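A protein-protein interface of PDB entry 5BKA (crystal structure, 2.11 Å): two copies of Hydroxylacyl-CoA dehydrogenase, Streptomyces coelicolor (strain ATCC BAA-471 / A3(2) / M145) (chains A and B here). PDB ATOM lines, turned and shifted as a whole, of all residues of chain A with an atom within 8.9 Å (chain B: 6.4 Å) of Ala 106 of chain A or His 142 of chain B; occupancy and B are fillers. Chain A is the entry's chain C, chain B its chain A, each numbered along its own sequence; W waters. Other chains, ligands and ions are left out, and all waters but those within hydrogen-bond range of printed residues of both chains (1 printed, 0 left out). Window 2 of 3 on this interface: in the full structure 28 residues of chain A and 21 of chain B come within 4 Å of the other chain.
CE2 of Phe 144 of chain B touches O of Ala 71 of chain A (3.5 Å).
Phe 144 of chain B touches Lys 73 of chain A (CZ to C, 3.8 Å).
Ile 74 of chain A touches Phe 144 of chain B (N to CZ, 3.8 Å).
Val 104 of chain A touches Asp 141 of chain B (CG1 to C, 3.6 Å).
His 142 of chain B touches Val 104 of chain A.
O of His 105 of chain A touches CB of His 142 of chain B, 3.4 Å away.
C of Ala 106 of chain A touches O of His 142 of chain B, at 3.5 Å.
Ala 106 of chain A touches Phe 144 of chain B (CB to CD1, 3.6 Å).
His 142 of chain B touches Val 108 of chain A.
Lys 109 of chain A touches His 142 of chain B.
O of His 142 of chain B is in hydrogen-bond range of N of Asp 107 of chain A.
The guanidinium group (NH2) of Arg 77 of chain A is in salt-bridge range of the side-chain carboxylate (OD1) of Asp 141 of chain B (2.9 Å).
Of the 15 printed residues of chain A, 11 touch a printed residue of chain B.
Of the 7 printed residues of chain B, 5 touch a printed residue of chain A.
Among the printed residues, Asp or Glu carboxylates within 4 Å of a Lys or Arg side-chain nitrogen of the other chain: Arg 77 of chain A with Asp 141 of chain B.
Water W1 lies within hydrogen-bond range of the backbone NH of Ser 116 of chain B (2.8 Å), a ring nitrogen (ND1) of His 142 of chain B (2.9 Å) and the backbone carbonyl oxygen of Lys 109 of chain A (3.0 Å).
The backbone carbonyl oxygen (O) of Lys 73 of chain A is in hydrogen-bond range of the backbone NH (N) of Ala 106 of chain A (3.0 Å).
The backbone NH (N) of Val 104 of chain A is in hydrogen-bond range of the backbone carbonyl oxygen (O) of Gln 75 of chain A (2.8 Å).
The side-chain hydroxyl (OG) of Ser 116 of chain B sits at hydrogen-bond distance from the side-chain carboxylate (OD2) of Asp 141 of chain B, at 2.6 Å.
The side-chain amide nitrogen (NE2) of Gln 75 of chain A lies close to the guanidinium group (NH1) of Arg 77 of chain A, 3.4 Å away.
Ala 106 of chain A touches just these residues of chain B: His 142 and Phe 144.
Of the printed residues of chain A, His 142 of chain B touches Val 104 (3.5 Å), His 105 (3.4 Å), Ala 106 (3.5 Å), Asp 107 (2.6 Å), Val 108 (3.1 Å) and Lys 109 (3.9 Å).
No residue of chain A comes within 4 Å of Val 143 of chain B.
Of the printed residues of chain A, Phe 144 of chain B touches Ala 71 (3.5 Å), Arg 72 (3.5 Å), Lys 73 (3.8 Å), Ile 74 (3.8 Å) and Ala 106 (3.6 Å).
Printed residues of chain B within 4 Å of Ala 71 of chain A: Phe 144 (3.5 Å).
Of the printed residues of chain B, His 105 of chain A touches His 142 (3.4 Å).
His 140 of chain B touches none of the printed residues of chain A.
Gln 75 of chain A touches none of the printed residues of chain B.
The nearest residue of chain A that does not touch His 142 of chain B is Gln 75 of chain A (6.0 Å).
No position is printed for both chains.
Of the 15 pairs that touch across the chains among the printed residues, none has its exchanged pair printed and touching as well.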
ATOM      1  N   ALA A  71       5.836 -12.046 -27.803  1.00  0.00           N
ATOM      2  CA  ALA A  71       7.128 -12.630 -27.459  1.00  0.00           C
ATOM      3  C   ALA A  71       7.052 -13.345 -26.115  1.00  0.00           C
ATOM      4  O   ALA A  71       7.934 -14.131 -25.767  1.00  0.00           O
ATOM      5  CB  ALA A  71       8.206 -11.559 -27.433  1.00  0.00           C
ATOM      6  N   ARG A  72       5.986 -13.061 -25.363  1.00  0.00           N
ATOM      7  CA  ARG A  72       5.801 -13.689 -24.059  1.00  0.00           C
ATOM      8  C   ARG A  72       5.518 -15.180 -24.185  1.00  0.00           C
ATOM      9  O   ARG A  72       5.825 -15.948 -23.266  1.00  0.00           O
ATOM     10  CB  ARG A  72       4.658 -13.009 -23.306  1.00  0.00           C
ATOM     11  CG  ARG A  72       5.070 -11.785 -22.513  1.00  0.00           C
ATOM     12  CD  ARG A  72       5.513 -12.170 -21.111  1.00  0.00           C
ATOM     13  NE  ARG A  72       5.673 -11.007 -20.240  1.00  0.00           N
ATOM     14  CZ  ARG A  72       6.655 -10.117 -20.343  1.00  0.00           C
ATOM     15  NH1 ARG A  72       7.587 -10.249 -21.279  1.00  0.00           N
ATOM     16  NH2 ARG A  72       6.712  -9.093 -19.502  1.00  0.00           N
ATOM     17  N   LYS A  73       4.937 -15.608 -25.305  1.00  0.00           N
ATOM     18  CA  LYS A  73       4.506 -16.989 -25.452  1.00  0.00           C
ATOM     19  C   LYS A  73       4.860 -17.610 -26.797  1.00  0.00           C
ATOM     20  O   LYS A  73       4.547 -18.786 -27.007  1.00  0.00           O
ATOM     21  CB  LYS A  73       2.987 -17.096 -25.232  1.00  0.00           C
ATOM     22  N   ILE A  74       5.498 -16.875 -27.708  1.00  0.00           N
ATOM     23  CA  ILE A  74       5.771 -17.362 -29.054  1.00  0.00           C
ATOM     24  C   ILE A  74       7.249 -17.177 -29.366  1.00  0.00           C
ATOM     25  O   ILE A  74       7.836 -16.138 -29.048  1.00  0.00           O
ATOM     26  CB  ILE A  74       4.907 -16.634 -30.108  1.00  0.00           C
ATOM     27  CG1 ILE A  74       3.429 -16.677 -29.719  1.00  0.00           C
ATOM     28  CG2 ILE A  74       5.116 -17.242 -31.485  1.00  0.00           C
ATOM     29  CD1 ILE A  74       2.788 -18.023 -29.930  1.00  0.00           C
ATOM     30  N   GLN A  75       7.845 -18.189 -29.997  1.00  0.00           N
ATOM     31  CA  GLN A  75       9.211 -18.120 -30.505  1.00  0.00           C
ATOM     32  C   GLN A  75       9.228 -18.655 -31.929  1.00  0.00           C
ATOM     33  O   GLN A  75       8.887 -19.819 -32.160  1.00  0.00           O
ATOM     34  CB  GLN A  75      10.177 -18.916 -29.623  1.00  0.00           C
ATOM     35  CG  GLN A  75      11.574 -19.050 -30.210  1.00  0.00           C
ATOM     36  CD  GLN A  75      12.312 -17.724 -30.271  1.00  0.00           C
ATOM     37  OE1 GLN A  75      12.556 -17.088 -29.246  1.00  0.00           O
ATOM     38  NE2 GLN A  75      12.669 -17.300 -31.478  1.00  0.00           N
ATOM     39  N   ARG A  77      11.127 -19.483 -35.694  1.00  0.00           N
ATOM     40  CA  ARG A  77      12.385 -19.910 -36.297  1.00  0.00           C
ATOM     41  C   ARG A  77      12.198 -20.014 -37.802  1.00  0.00           C
ATOM     42  O   ARG A  77      11.288 -20.707 -38.268  1.00  0.00           O
ATOM     43  CB  ARG A  77      12.856 -21.258 -35.734  1.00  0.00           C
ATOM     44  CG  ARG A  77      13.140 -21.260 -34.238  1.00  0.00           C
ATOM     45  CD  ARG A  77      14.378 -20.446 -33.893  1.00  0.00           C
ATOM     46  NE  ARG A  77      14.599 -20.392 -32.449  1.00  0.00           N
ATOM     47  CZ  ARG A  77      15.254 -19.418 -31.825  1.00  0.00           C
ATOM     48  NH1 ARG A  77      15.762 -18.406 -32.514  1.00  0.00           N
ATOM     49  NH2 ARG A  77      15.402 -19.457 -30.508  1.00  0.00           N
ATOM     50  N   THR A 103       6.744 -22.100 -35.628  1.00  0.00           N
ATOM     51  CA  THR A 103       6.139 -21.319 -34.554  1.00  0.00           C
ATOM     52  C   THR A 103       6.112 -22.184 -33.300  1.00  0.00           C
ATOM     53  O   THR A 103       5.378 -23.177 -33.241  1.00  0.00           O
ATOM     54  CB  THR A 103       4.737 -20.847 -34.931  1.00  0.00           C
ATOM     55  OG1 THR A 103       4.802 -20.074 -36.136  1.00  0.00           O
ATOM     56  CG2 THR A 103       4.148 -19.990 -33.820  1.00  0.00           C
ATOM     57  N   VAL A 104       6.917 -21.820 -32.307  1.00  0.00           N
ATOM     58  CA  VAL A 104       7.045 -22.587 -31.074  1.00  0.00           C
ATOM     59  C   VAL A 104       6.256 -21.885 -29.979  1.00  0.00           C
ATOM     60  O   VAL A 104       6.494 -20.705 -29.690  1.00  0.00           O
ATOM     61  CB  VAL A 104       8.517 -22.762 -30.669  1.00  0.00           C
ATOM     62  CG1 VAL A 104       8.617 -23.602 -29.406  1.00  0.00           C
ATOM     63  CG2 VAL A 104       9.311 -23.397 -31.802  1.00  0.00           C
ATOM     64  N   HIS A 105       5.313 -22.606 -29.378  1.00  0.00           N
ATOM     65  CA  HIS A 105       4.487 -22.098 -28.292  1.00  0.00           C
ATOM     66  C   HIS A 105       5.082 -22.504 -26.951  1.00  0.00           C
ATOM     67  O   HIS A 105       5.669 -23.583 -26.823  1.00  0.00           O
ATOM     68  CB  HIS A 105       3.055 -22.622 -28.402  1.00  0.00           C
ATOM     69  CG  HIS A 105       2.322 -22.129 -29.609  1.00  0.00           C
ATOM     70  ND1 HIS A 105       1.503 -21.021 -29.580  1.00  0.00           N
ATOM     71  CD2 HIS A 105       2.281 -22.595 -30.880  1.00  0.00           C
ATOM     72  CE1 HIS A 105       0.991 -20.824 -30.782  1.00  0.00           C
ATOM     73  NE2 HIS A 105       1.447 -21.766 -31.589  1.00  0.00           N
ATOM     74  N   ALA A 106       4.946 -21.620 -25.963  1.00  0.00           N
ATOM     75  CA  ALA A 106       5.421 -21.904 -24.614  1.00  0.00           C
ATOM     76  C   ALA A 106       4.864 -23.227 -24.102  1.00  0.00           C
ATOM     77  O   ALA A 106       3.660 -23.486 -24.194  1.00  0.00           O
ATOM     78  CB  ALA A 106       5.024 -20.766 -23.670  1.00  0.00           C
ATOM     79  N   ASP A 107       5.759 -24.068 -23.581  1.00  0.00           N
ATOM     80  CA  ASP A 107       5.419 -25.352 -22.965  1.00  0.00           C
ATOM     81  C   ASP A 107       4.818 -26.345 -23.956  1.00  0.00           C
ATOM     82  O   ASP A 107       4.154 -27.303 -23.549  1.00  0.00           O
ATOM     83  CB  ASP A 107       4.477 -25.170 -21.769  1.00  0.00           C
ATOM     84  CG  ASP A 107       5.062 -24.269 -20.701  1.00  0.00           C
ATOM     85  OD1 ASP A 107       6.300 -24.271 -20.527  1.00  0.00           O
ATOM     86  OD2 ASP A 107       4.283 -23.557 -20.035  1.00  0.00           O
ATOM     87  N   VAL A 108       5.036 -26.146 -25.254  1.00  0.00           N
ATOM     88  CA  VAL A 108       4.573 -27.075 -26.279  1.00  0.00           C
ATOM     89  C   VAL A 108       5.794 -27.530 -27.063  1.00  0.00           C
ATOM     90  O   VAL A 108       6.403 -26.736 -27.792  1.00  0.00           O
ATOM     91  CB  VAL A 108       3.529 -26.440 -27.208  1.00  0.00           C
ATOM     92  CG1 VAL A 108       3.029 -27.457 -28.226  1.00  0.00           C
ATOM     93  CG2 VAL A 108       2.376 -25.866 -26.403  1.00  0.00           C
ATOM     94  N   LYS A 109       6.125 -28.818 -26.952  1.00  0.00           N
ATOM     95  CA  LYS A 109       7.373 -29.311 -27.524  1.00  0.00           C
ATOM     96  C   LYS A 109       7.304 -29.363 -29.045  1.00  0.00           C
ATOM     97  O   LYS A 109       8.284 -29.042 -29.725  1.00  0.00           O
ATOM     98  CB  LYS A 109       7.694 -30.695 -26.956  1.00  0.00           C
ATOM     99  CG  LYS A 109       8.954 -31.325 -27.525  1.00  0.00           C
ATOM    100  CD  LYS A 109       9.344 -32.583 -26.764  1.00  0.00           C
ATOM    101  CE  LYS A 109       8.350 -33.710 -27.005  1.00  0.00           C
ATOM    102  NZ  LYS A 109       7.881 -34.321 -25.729  1.00  0.00           N
ATOM    103  N   ALA A 110       6.153 -29.739 -29.591  1.00  0.00           N
ATOM    104  CA  ALA A 110       5.996 -29.830 -31.039  1.00  0.00           C
ATOM    105  C   ALA A 110       5.735 -28.454 -31.629  1.00  0.00           C
ATOM    106  O   ALA A 110       4.744 -27.808 -31.263  1.00  0.00           O
ATOM    107  CB  ALA A 110       4.853 -30.775 -31.391  1.00  0.00           C
ATOM    108  N   PRO A 111       6.575 -27.965 -32.537  1.00  0.00           N
ATOM    109  CA  PRO A 111       6.300 -26.682 -33.187  1.00  0.00           C
ATOM    110  C   PRO A 111       5.148 -26.790 -34.175  1.00  0.00           C
ATOM    111  O   PRO A 111       4.798 -27.869 -34.659  1.00  0.00           O
ATOM    112  CB  PRO A 111       7.613 -26.351 -33.910  1.00  0.00           C
ATOM    113  CG  PRO A 111       8.621 -27.360 -33.428  1.00  0.00           C
ATOM    114  CD  PRO A 111       7.842 -28.558 -32.996  1.00  0.00           C
ATOM    115  N   PRO B 115      11.886 -31.563 -29.577  1.00  0.00           N
ATOM    116  CA  PRO B 115      11.800 -30.109 -29.405  1.00  0.00           C
ATOM    117  C   PRO B 115      12.572 -29.327 -30.469  1.00  0.00           C
ATOM    118  O   PRO B 115      13.398 -29.917 -31.182  1.00  0.00           O
ATOM    119  CB  PRO B 115      12.416 -29.897 -28.021  1.00  0.00           C
ATOM    120  CG  PRO B 115      13.440 -30.980 -27.925  1.00  0.00           C
ATOM    121  CD  PRO B 115      12.878 -32.168 -28.667  1.00  0.00           C
ATOM    122  N   SER B 116      12.273 -28.034 -30.591  1.00  0.00           N
ATOM    123  CA  SER B 116      13.116 -27.108 -31.333  1.00  0.00           C
ATOM    124  C   SER B 116      14.086 -26.461 -30.353  1.00  0.00           C
ATOM    125  O   SER B 116      13.668 -25.950 -29.310  1.00  0.00           O
ATOM    126  CB  SER B 116      12.261 -26.057 -32.041  1.00  0.00           C
ATOM    127  OG  SER B 116      13.005 -24.937 -32.476  1.00  0.00           O
ATOM    128  N   HIS B 140      15.698 -25.120 -24.937  1.00  0.00           N
ATOM    129  CA  HIS B 140      14.498 -25.524 -25.651  1.00  0.00           C
ATOM    130  C   HIS B 140      13.642 -24.298 -25.927  1.00  0.00           C
ATOM    131  O   HIS B 140      13.383 -23.499 -25.022  1.00  0.00           O
ATOM    132  CB  HIS B 140      13.713 -26.562 -24.849  1.00  0.00           C
ATOM    133  CG  HIS B 140      14.504 -27.785 -24.505  1.00  0.00           C
ATOM    134  ND1 HIS B 140      15.545 -28.244 -25.283  1.00  0.00           N
ATOM    135  CD2 HIS B 140      14.406 -28.644 -23.463  1.00  0.00           C
ATOM    136  CE1 HIS B 140      16.053 -29.334 -24.736  1.00  0.00           C
ATOM    137  NE2 HIS B 140      15.380 -29.599 -23.631  1.00  0.00           N
ATOM    138  N   ASP B 141      13.215 -24.153 -27.182  1.00  0.00           N
ATOM    139  CA  ASP B 141      12.477 -22.963 -27.588  1.00  0.00           C
ATOM    140  C   ASP B 141      11.122 -22.872 -26.898  1.00  0.00           C
ATOM    141  O   ASP B 141      10.571 -21.773 -26.769  1.00  0.00           O
ATOM    142  CB  ASP B 141      12.304 -22.945 -29.107  1.00  0.00           C
ATOM    143  CG  ASP B 141      13.571 -22.540 -29.835  1.00  0.00           C
ATOM    144  OD1 ASP B 141      14.423 -21.863 -29.221  1.00  0.00           O
ATOM    145  OD2 ASP B 141      13.718 -22.900 -31.021  1.00  0.00           O
ATOM    146  N   HIS B 142      10.559 -24.001 -26.470  1.00  0.00           N
ATOM    147  CA  HIS B 142       9.265 -23.999 -25.800  1.00  0.00           C
ATOM    148  C   HIS B 142       9.364 -23.773 -24.294  1.00  0.00           C
ATOM    149  O   HIS B 142       8.326 -23.655 -23.634  1.00  0.00           O
ATOM    150  CB  HIS B 142       8.520 -25.309 -26.077  1.00  0.00           C
ATOM    151  CG  HIS B 142       9.165 -26.520 -25.478  1.00  0.00           C
ATOM    152  ND1 HIS B 142      10.316 -27.081 -25.989  1.00  0.00           N
ATOM    153  CD2 HIS B 142       8.807 -27.291 -24.425  1.00  0.00           C
ATOM    154  CE1 HIS B 142      10.645 -28.139 -25.270  1.00  0.00           C
ATOM    155  NE2 HIS B 142       9.746 -28.288 -24.314  1.00  0.00           N
ATOM    156  N   VAL B 143      10.569 -23.696 -23.740  1.00  0.00           N
ATOM    157  CA  VAL B 143      10.768 -23.436 -22.319  1.00  0.00           C
ATOM    158  C   VAL B 143      11.095 -21.957 -22.164  1.00  0.00           C
ATOM    159  O   VAL B 143      12.181 -21.507 -22.544  1.00  0.00           O
ATOM    160  CB  VAL B 143      11.873 -24.319 -21.725  1.00  0.00           C
ATOM    161  CG1 VAL B 143      11.902 -24.181 -20.210  1.00  0.00           C
ATOM    162  CG2 VAL B 143      11.652 -25.767 -22.113  1.00  0.00           C
ATOM    163  N   PHE B 144      10.153 -21.202 -21.607  1.00  0.00           N
ATOM    164  CA  PHE B 144      10.295 -19.767 -21.431  1.00  0.00           C
ATOM    165  C   PHE B 144      10.659 -19.435 -19.987  1.00  0.00           C
ATOM    166  O   PHE B 144      10.288 -20.164 -19.063  1.00  0.00           O
ATOM    167  CB  PHE B 144       8.996 -19.051 -21.811  1.00  0.00           C
ATOM    168  CG  PHE B 144       8.785 -18.928 -23.294  1.00  0.00           C
ATOM    169  CD1 PHE B 144       8.570 -20.052 -24.073  1.00  0.00           C
ATOM    170  CD2 PHE B 144       8.802 -17.687 -23.909  1.00  0.00           C
ATOM    171  CE1 PHE B 144       8.377 -19.943 -25.436  1.00  0.00           C
ATOM    172  CE2 PHE B 144       8.608 -17.571 -25.273  1.00  0.00           C
ATOM    173  CZ  PHE B 144       8.397 -18.702 -26.037  1.00  0.00           C
HETATM  174  O   HOH W   1      10.324 -26.992 -28.932  1.00  0.00           O
